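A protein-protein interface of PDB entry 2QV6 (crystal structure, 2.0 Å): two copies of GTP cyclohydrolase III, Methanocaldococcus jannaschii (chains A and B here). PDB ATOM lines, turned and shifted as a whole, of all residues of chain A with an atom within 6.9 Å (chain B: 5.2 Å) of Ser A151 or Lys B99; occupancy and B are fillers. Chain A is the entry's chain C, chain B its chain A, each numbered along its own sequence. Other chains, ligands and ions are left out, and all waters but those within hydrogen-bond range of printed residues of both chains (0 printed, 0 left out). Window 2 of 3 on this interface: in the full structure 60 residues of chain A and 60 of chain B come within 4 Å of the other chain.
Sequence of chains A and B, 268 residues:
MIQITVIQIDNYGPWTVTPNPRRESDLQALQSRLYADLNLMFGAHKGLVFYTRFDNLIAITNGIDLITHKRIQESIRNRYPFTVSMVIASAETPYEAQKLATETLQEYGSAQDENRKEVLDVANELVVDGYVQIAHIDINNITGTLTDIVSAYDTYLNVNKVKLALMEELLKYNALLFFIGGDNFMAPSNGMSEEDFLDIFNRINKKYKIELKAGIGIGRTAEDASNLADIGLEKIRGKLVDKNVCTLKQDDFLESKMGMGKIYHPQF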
ATOM      1  N   LEU A 146      11.900  -3.533   4.455  1.00  0.00           N
ATOM      2  CA  LEU A 146      10.904  -4.065   3.508  1.00  0.00           C
ATOM      3  C   LEU A 146      10.055  -5.212   4.058  1.00  0.00           C
ATOM      4  O   LEU A 146       8.826  -5.129   4.076  1.00  0.00           O
ATOM      5  CB  LEU A 146      11.582  -4.474   2.202  1.00  0.00           C
ATOM      6  CG  LEU A 146      12.082  -3.309   1.340  1.00  0.00           C
ATOM      7  CD1 LEU A 146      12.836  -3.843   0.136  1.00  0.00           C
ATOM      8  CD2 LEU A 146      10.936  -2.401   0.905  1.00  0.00           C
ATOM      9  N   THR A 147      10.703  -6.275   4.521  1.00  0.00           N
ATOM     10  CA  THR A 147       9.974  -7.483   4.906  1.00  0.00           C
ATOM     11  C   THR A 147       8.949  -7.223   5.991  1.00  0.00           C
ATOM     12  O   THR A 147       7.830  -7.751   5.921  1.00  0.00           O
ATOM     13  CB  THR A 147      10.904  -8.607   5.410  1.00  0.00           C
ATOM     14  OG1 THR A 147      11.990  -8.786   4.496  1.00  0.00           O
ATOM     15  CG2 THR A 147      10.123  -9.909   5.548  1.00  0.00           C
ATOM     16  N   ILE A 149       7.616  -4.287   6.712  1.00  0.00           N
ATOM     17  CA  ILE A 149       6.963  -2.982   6.459  1.00  0.00           C
ATOM     18  C   ILE A 149       5.942  -2.945   5.304  1.00  0.00           C
ATOM     19  O   ILE A 149       4.847  -2.375   5.460  1.00  0.00           O
ATOM     20  CB  ILE A 149       8.003  -1.892   6.131  1.00  0.00           C
ATOM     21  CG1 ILE A 149       9.139  -1.904   7.143  1.00  0.00           C
ATOM     22  CG2 ILE A 149       7.339  -0.508   6.077  1.00  0.00           C
ATOM     23  CD1 ILE A 149       8.734  -1.555   8.544  1.00  0.00           C
ATOM     24  N   VAL A 150       6.315  -3.508   4.151  1.00  0.00           N
ATOM     25  CA  VAL A 150       5.468  -3.533   2.949  1.00  0.00           C
ATOM     26  C   VAL A 150       4.952  -4.952   2.689  1.00  0.00           C
ATOM     27  O   VAL A 150       5.304  -5.880   3.415  1.00  0.00           O
ATOM     28  CB  VAL A 150       6.199  -2.953   1.721  1.00  0.00           C
ATOM     29  CG1 VAL A 150       6.675  -1.559   2.033  1.00  0.00           C
ATOM     30  CG2 VAL A 150       7.389  -3.828   1.293  1.00  0.00           C
ATOM     31  N   SER A 151       4.092  -5.119   1.687  1.00  0.00           N
ATOM     32  CA  SER A 151       3.450  -6.414   1.453  1.00  0.00           C
ATOM     33  C   SER A 151       4.476  -7.389   0.894  1.00  0.00           C
ATOM     34  O   SER A 151       5.546  -6.976   0.438  1.00  0.00           O
ATOM     35  CB  SER A 151       2.260  -6.297   0.500  1.00  0.00           C
ATOM     36  OG  SER A 151       2.658  -6.149  -0.858  1.00  0.00           O
ATOM     37  N   ALA A 152       4.148  -8.671   0.959  1.00  0.00           N
ATOM     38  CA  ALA A 152       5.026  -9.728   0.444  1.00  0.00           C
ATOM     39  C   ALA A 152       5.362  -9.492  -1.021  1.00  0.00           C
ATOM     40  O   ALA A 152       6.545  -9.596  -1.430  1.00  0.00           O
ATOM     41  CB  ALA A 152       4.375 -11.080   0.641  1.00  0.00           C
ATOM     42  N   TYR A 153       4.348  -9.120  -1.809  1.00  0.00           N
ATOM     43  CA  TYR A 153       4.531  -8.939  -3.236  1.00  0.00           C
ATOM     44  C   TYR A 153       5.377  -7.701  -3.523  1.00  0.00           C
ATOM     45  O   TYR A 153       6.155  -7.720  -4.467  1.00  0.00           O
ATOM     46  CB  TYR A 153       3.198  -8.897  -4.021  1.00  0.00           C
ATOM     47  CG  TYR A 153       3.372  -9.063  -5.517  1.00  0.00           C
ATOM     48  CD1 TYR A 153       3.695 -10.311  -6.068  1.00  0.00           C
ATOM     49  CD2 TYR A 153       3.262  -7.978  -6.380  1.00  0.00           C
ATOM     50  CE1 TYR A 153       3.888 -10.467  -7.435  1.00  0.00           C
ATOM     51  CE2 TYR A 153       3.440  -8.120  -7.742  1.00  0.00           C
ATOM     52  CZ  TYR A 153       3.756  -9.366  -8.267  1.00  0.00           C
ATOM     53  OH  TYR A 153       3.933  -9.501  -9.616  1.00  0.00           O
ATOM     54  N   ASP A 154       5.235  -6.651  -2.702  1.00  0.00           N
ATOM     55  CA  ASP A 154       6.043  -5.445  -2.855  1.00  0.00           C
ATOM     56  C   ASP A 154       7.523  -5.701  -2.588  1.00  0.00           C
ATOM     57  O   ASP A 154       8.371  -5.170  -3.283  1.00  0.00           O
ATOM     58  CB  ASP A 154       5.535  -4.309  -1.941  1.00  0.00           C
ATOM     59  CG  ASP A 154       4.203  -3.741  -2.388  1.00  0.00           C
ATOM     60  OD1 ASP A 154       4.050  -3.372  -3.551  1.00  0.00           O
ATOM     61  OD2 ASP A 154       3.287  -3.656  -1.568  1.00  0.00           O
ATOM     62  N   THR A 155       7.854  -6.497  -1.584  1.00  0.00           N
ATOM     63  CA  THR A 155       9.277  -6.833  -1.352  1.00  0.00           C
ATOM     64  C   THR A 155       9.831  -7.672  -2.507  1.00  0.00           C
ATOM     65  O   THR A 155      10.965  -7.502  -2.951  1.00  0.00           O
ATOM     66  CB  THR A 155       9.450  -7.559  -0.020  1.00  0.00           C
ATOM     67  OG1 THR A 155       8.858  -6.767   1.015  1.00  0.00           O
ATOM     68  CG2 THR A 155      10.910  -7.799   0.319  1.00  0.00           C
ATOM     69  N   TYR A 156       9.011  -8.571  -3.011  1.00  0.00           N
ATOM     70  CA  TYR A 156       9.341  -9.390  -4.187  1.00  0.00           C
ATOM     71  C   TYR A 156       9.626  -8.586  -5.466  1.00  0.00           C
ATOM     72  O   TYR A 156      10.542  -8.904  -6.212  1.00  0.00           O
ATOM     73  CB  TYR A 156       8.187 -10.381  -4.395  1.00  0.00           C
ATOM     74  CG  TYR A 156       8.061 -11.063  -5.721  1.00  0.00           C
ATOM     75  CD1 TYR A 156       8.876 -12.138  -6.043  1.00  0.00           C
ATOM     76  CD2 TYR A 156       7.035 -10.704  -6.620  1.00  0.00           C
ATOM     77  CE1 TYR A 156       8.718 -12.829  -7.260  1.00  0.00           C
ATOM     78  CE2 TYR A 156       6.870 -11.380  -7.827  1.00  0.00           C
ATOM     79  CZ  TYR A 156       7.725 -12.449  -8.146  1.00  0.00           C
ATOM     80  OH  TYR A 156       7.556 -13.126  -9.346  1.00  0.00           O
ATOM     81  N   PRO B  94      -5.991 -10.340  -6.553  1.00  0.00           N
ATOM     82  CA  PRO B  94      -4.836 -10.939  -5.903  1.00  0.00           C
ATOM     83  C   PRO B  94      -3.971  -9.981  -5.050  1.00  0.00           C
ATOM     84  O   PRO B  94      -3.493 -10.358  -3.992  1.00  0.00           O
ATOM     85  CB  PRO B  94      -4.007 -11.456  -7.085  1.00  0.00           C
ATOM     86  CG  PRO B  94      -4.983 -11.678  -8.161  1.00  0.00           C
ATOM     87  CD  PRO B  94      -6.030 -10.643  -7.992  1.00  0.00           C
ATOM     88  N   TYR B  95      -3.753  -8.768  -5.526  1.00  0.00           N
ATOM     89  CA  TYR B  95      -2.852  -7.848  -4.849  1.00  0.00           C
ATOM     90  C   TYR B  95      -3.477  -7.416  -3.531  1.00  0.00           C
ATOM     91  O   TYR B  95      -2.797  -7.392  -2.513  1.00  0.00           O
ATOM     92  CB  TYR B  95      -2.496  -6.645  -5.743  1.00  0.00           C
ATOM     93  CG  TYR B  95      -1.598  -5.666  -5.035  1.00  0.00           C
ATOM     94  CD1 TYR B  95      -0.216  -5.772  -5.116  1.00  0.00           C
ATOM     95  CD2 TYR B  95      -2.136  -4.664  -4.226  1.00  0.00           C
ATOM     96  CE1 TYR B  95       0.616  -4.905  -4.418  1.00  0.00           C
ATOM     97  CE2 TYR B  95      -1.319  -3.796  -3.517  1.00  0.00           C
ATOM     98  CZ  TYR B  95       0.057  -3.915  -3.627  1.00  0.00           C
ATOM     99  OH  TYR B  95       0.856  -3.047  -2.928  1.00  0.00           O
ATOM    100  N   GLU B  96      -4.780  -7.104  -3.544  1.00  0.00           N
ATOM    101  CA  GLU B  96      -5.528  -6.797  -2.306  1.00  0.00           C
ATOM    102  C   GLU B  96      -5.386  -7.935  -1.293  1.00  0.00           C
ATOM    103  O   GLU B  96      -5.044  -7.701  -0.136  1.00  0.00           O
ATOM    104  CB  GLU B  96      -7.028  -6.590  -2.575  1.00  0.00           C
ATOM    105  CG  GLU B  96      -7.445  -5.302  -3.289  1.00  0.00           C
ATOM    106  CD  GLU B  96      -8.896  -5.387  -3.867  1.00  0.00           C
ATOM    107  OE1 GLU B  96      -9.842  -5.744  -3.105  1.00  0.00           O
ATOM    108  OE2 GLU B  96      -9.080  -5.109  -5.087  1.00  0.00           O
ATOM    109  N   ALA B  97      -5.650  -9.157  -1.759  1.00  0.00           N
ATOM    110  CA  ALA B  97      -5.592 -10.375  -0.937  1.00  0.00           C
ATOM    111  C   ALA B  97      -4.257 -10.579  -0.187  1.00  0.00           C
ATOM    112  O   ALA B  97      -4.249 -10.810   1.022  1.00  0.00           O
ATOM    113  CB  ALA B  97      -5.913 -11.597  -1.810  1.00  0.00           C
ATOM    114  N   GLN B  98      -3.135 -10.502  -0.897  1.00  0.00           N
ATOM    115  CA  GLN B  98      -1.830 -10.739  -0.256  1.00  0.00           C
ATOM    116  C   GLN B  98      -1.401  -9.605   0.648  1.00  0.00           C
ATOM    117  O   GLN B  98      -0.678  -9.829   1.615  1.00  0.00           O
ATOM    118  CB  GLN B  98      -0.718 -11.073  -1.274  1.00  0.00           C
ATOM    119  CG  GLN B  98      -0.373 -10.033  -2.345  1.00  0.00           C
ATOM    120  CD  GLN B  98       0.577  -8.955  -1.875  1.00  0.00           C
ATOM    121  OE1 GLN B  98       0.436  -7.780  -2.248  1.00  0.00           O
ATOM    122  NE2 GLN B  98       1.533  -9.329  -1.048  1.00  0.00           N
ATOM    123  N   LYS B  99      -1.855  -8.395   0.337  1.00  0.00           N
ATOM    124  CA  LYS B  99      -1.542  -7.209   1.137  1.00  0.00           C
ATOM    125  C   LYS B  99      -2.202  -7.325   2.505  1.00  0.00           C
ATOM    126  O   LYS B  99      -1.555  -7.095   3.516  1.00  0.00           O
ATOM    127  CB  LYS B  99      -2.004  -5.939   0.409  1.00  0.00           C
ATOM    128  CG  LYS B  99      -1.746  -4.613   1.162  1.00  0.00           C
ATOM    129  CD  LYS B  99      -2.313  -3.439   0.379  1.00  0.00           C
ATOM    130  CE  LYS B  99      -1.720  -2.107   0.818  1.00  0.00           C
ATOM    131  NZ  LYS B  99      -1.841  -1.892   2.284  1.00  0.00           N
ATOM    132  N   LEU B 100      -3.486  -7.696   2.535  1.00  0.00           N
ATOM    133  CA  LEU B 100      -4.175  -7.967   3.796  1.00  0.00           C
ATOM    134  C   LEU B 100      -3.506  -9.104   4.582  1.00  0.00           C
ATOM    135  O   LEU B 100      -3.254  -8.956   5.779  1.00  0.00           O
ATOM    136  CB  LEU B 100      -5.645  -8.330   3.550  1.00  0.00           C
ATOM    137  CG  LEU B 100      -6.574  -7.263   2.981  1.00  0.00           C
ATOM    138  CD1 LEU B 100      -7.970  -7.846   2.894  1.00  0.00           C
ATOM    139  CD2 LEU B 100      -6.574  -6.015   3.846  1.00  0.00           C
ATOM    140  N   ALA B 101      -3.240 -10.245   3.921  1.00  0.00           N
ATOM    141  CA  ALA B 101      -2.560 -11.387   4.576  1.00  0.00           C
ATOM    142  C   ALA B 101      -1.243 -10.940   5.212  1.00  0.00           C
ATOM    143  O   ALA B 101      -0.941 -11.279   6.355  1.00  0.00           O
ATOM    144  CB  ALA B 101      -2.313 -12.541   3.579  1.00  0.00           C
ATOM    145  N   THR B 102      -0.459 -10.166   4.484  1.00  0.00           N
ATOM    146  CA  THR B 102       0.850  -9.759   4.997  1.00  0.00           C
ATOM    147  C   THR B 102       0.667  -8.814   6.189  1.00  0.00           C
ATOM    148  O   THR B 102       1.472  -8.815   7.124  1.00  0.00           O
ATOM    149  CB  THR B 102       1.734  -9.075   3.923  1.00  0.00           C
ATOM    150  OG1 THR B 102       1.769  -9.859   2.729  1.00  0.00           O
ATOM    151  CG2 THR B 102       3.137  -8.889   4.448  1.00  0.00           C
ATOM    152  N   GLU B 103      -0.391  -8.005   6.175  1.00  0.00           N
ATOM    153  CA  GLU B 103      -0.578  -7.017   7.251  1.00  0.00           C
ATOM    154  C   GLU B 103      -0.829  -7.685   8.578  1.00  0.00           C
ATOM    155  O   GLU B 103      -0.280  -7.272   9.589  1.00  0.00           O
ATOM    156  CB  GLU B 103      -1.721  -6.040   6.926  1.00  0.00           C
ATOM    157  CG  GLU B 103      -1.246  -4.829   6.144  1.00  0.00           C
ATOM    158  CD  GLU B 103      -2.331  -4.081   5.399  1.00  0.00           C
ATOM    159  OE1 GLU B 103      -3.552  -4.395   5.554  1.00  0.00           O
ATOM    160  OE2 GLU B 103      -1.926  -3.162   4.639  1.00  0.00           O
ATOM    161  N   GLN B 106       2.338  -9.277   9.999  1.00  0.00           N
ATOM    162  CA  GLN B 106       3.292  -8.313  10.565  1.00  0.00           C
ATOM    163  C   GLN B 106       2.823  -7.795  11.931  1.00  0.00           C
ATOM    164  O   GLN B 106       3.620  -7.454  12.787  1.00  0.00           O
ATOM    165  CB  GLN B 106       3.527  -7.158   9.582  1.00  0.00           C
ATOM    166  CG  GLN B 106       4.210  -7.566   8.273  1.00  0.00           C
ATOM    167  CD  GLN B 106       4.155  -6.505   7.177  1.00  0.00           C
ATOM    168  OE1 GLN B 106       5.102  -6.363   6.400  1.00  0.00           O
ATOM    169  NE2 GLN B 106       3.047  -5.767   7.098  1.00  0.00           N
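Printed residues of chain B that touch a printed residue of chain A: Tyr B95, Gln B98, Lys B99, Thr B102 and Gln B106.
Hydrophobic or aromatic side chains of chain B that line the printed part of chain A: Tyr B95.
Hydrophobic or aromatic side chains of chain A within 4 Å of the printed part of chain B: Ala A152 and Tyr A153.
Among the printed residues, no Asp or Glu carboxylate lies within 4 Å of a Lys or Arg side-chain nitrogen of the other chain.
No position is printed for both chains.
Of the 11 pairs that touch across the chains among the printed residues, none has its exchanged pair printed and touching as well.
Among the printed residues, merely in contact across the chains: Val A150 with Thr B102 (3.8 Å), Ser A151 with Thr B102 (3.9 Å) and Ser A151 with Lys B99 (3.96 Å).
The backbone carbonyl oxygen (O) of Tyr B95 lies close to the side-chain amide oxygen (OE1) of Gln B98 (3.3 Å).
OG1 of Thr B102 lies within hydrogen-bond range of O of Gln B98.
The side-chain carboxylate (OE2) of Glu B103 lies within salt-bridge range of the side-chain amino group (NZ) of Lys B99.
The side-chain amide nitrogen (NE2) of Gln B106 lies close to the backbone carbonyl oxygen (O) of Thr B102.
OG of Ser A151 lies within hydrogen-bond range of OD2 of Asp A154.
The backbone carbonyl oxygen of Ser A151 is in hydrogen-bond range of the side-chain hydroxyl of Thr A155 (3.4 Å).
Of the printed residues of chain B, Ser A151 touches Gln B98, Lys B99 and Thr B102.
Of the printed residues of chain A, Lys B99 touches Ser A151.
Of the printed residues of chain A, Gln B98 touches Ser A151, Ala A152 and Tyr A153.
Printed residues of chain A within 4 Å of Thr B102: Val A150, Ser A151 and Ala A152.
Of the printed residues of chain B, Asp A154 touches Tyr B95 (2.9 Å).
Printed residues of chain B within 4 Å of Thr A147: Gln B106.
Of the printed residues of chain B, Tyr A153 touches Gln B98.
The nearest residue of chain B that does not touch Ser A151 is Tyr B95 (4.1 Å).
The side-chain carboxylate (OD2) of Asp A154 lies within hydrogen-bond range of the side-chain hydroxyl (OH) of Tyr B95.
The side-chain amide oxygen (OE1) of Gln B98 sits at hydrogen-bond distance from the side-chain hydroxyl (OG) of Ser A151, at 3.1 Å.
The side-chain amide nitrogen (NE2) of Gln B98 lies close to the backbone NH (N) of Ala A152 (3.4 Å).
NE2 of Gln B98 lies close to N of Tyr A153 (2.9 Å).
The backbone NH (N) of Ala A152 sits at hydrogen-bond distance from the side-chain hydroxyl (OG1) of Thr B102, at 3.2 Å.
The side-chain amide oxygen of Gln B106 lies close to the backbone carbonyl oxygen of Thr A147, 3.1 Å away.
The backbone NH (N) of Ile A149 lies within hydrogen-bond range of the side-chain amide oxygen (OE1) of Gln B106 (3.3 Å).
The side-chain amide oxygen (OE1) of Gln B106 lies close to the backbone carbonyl oxygen (O) of Val A150 (3.0 Å).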
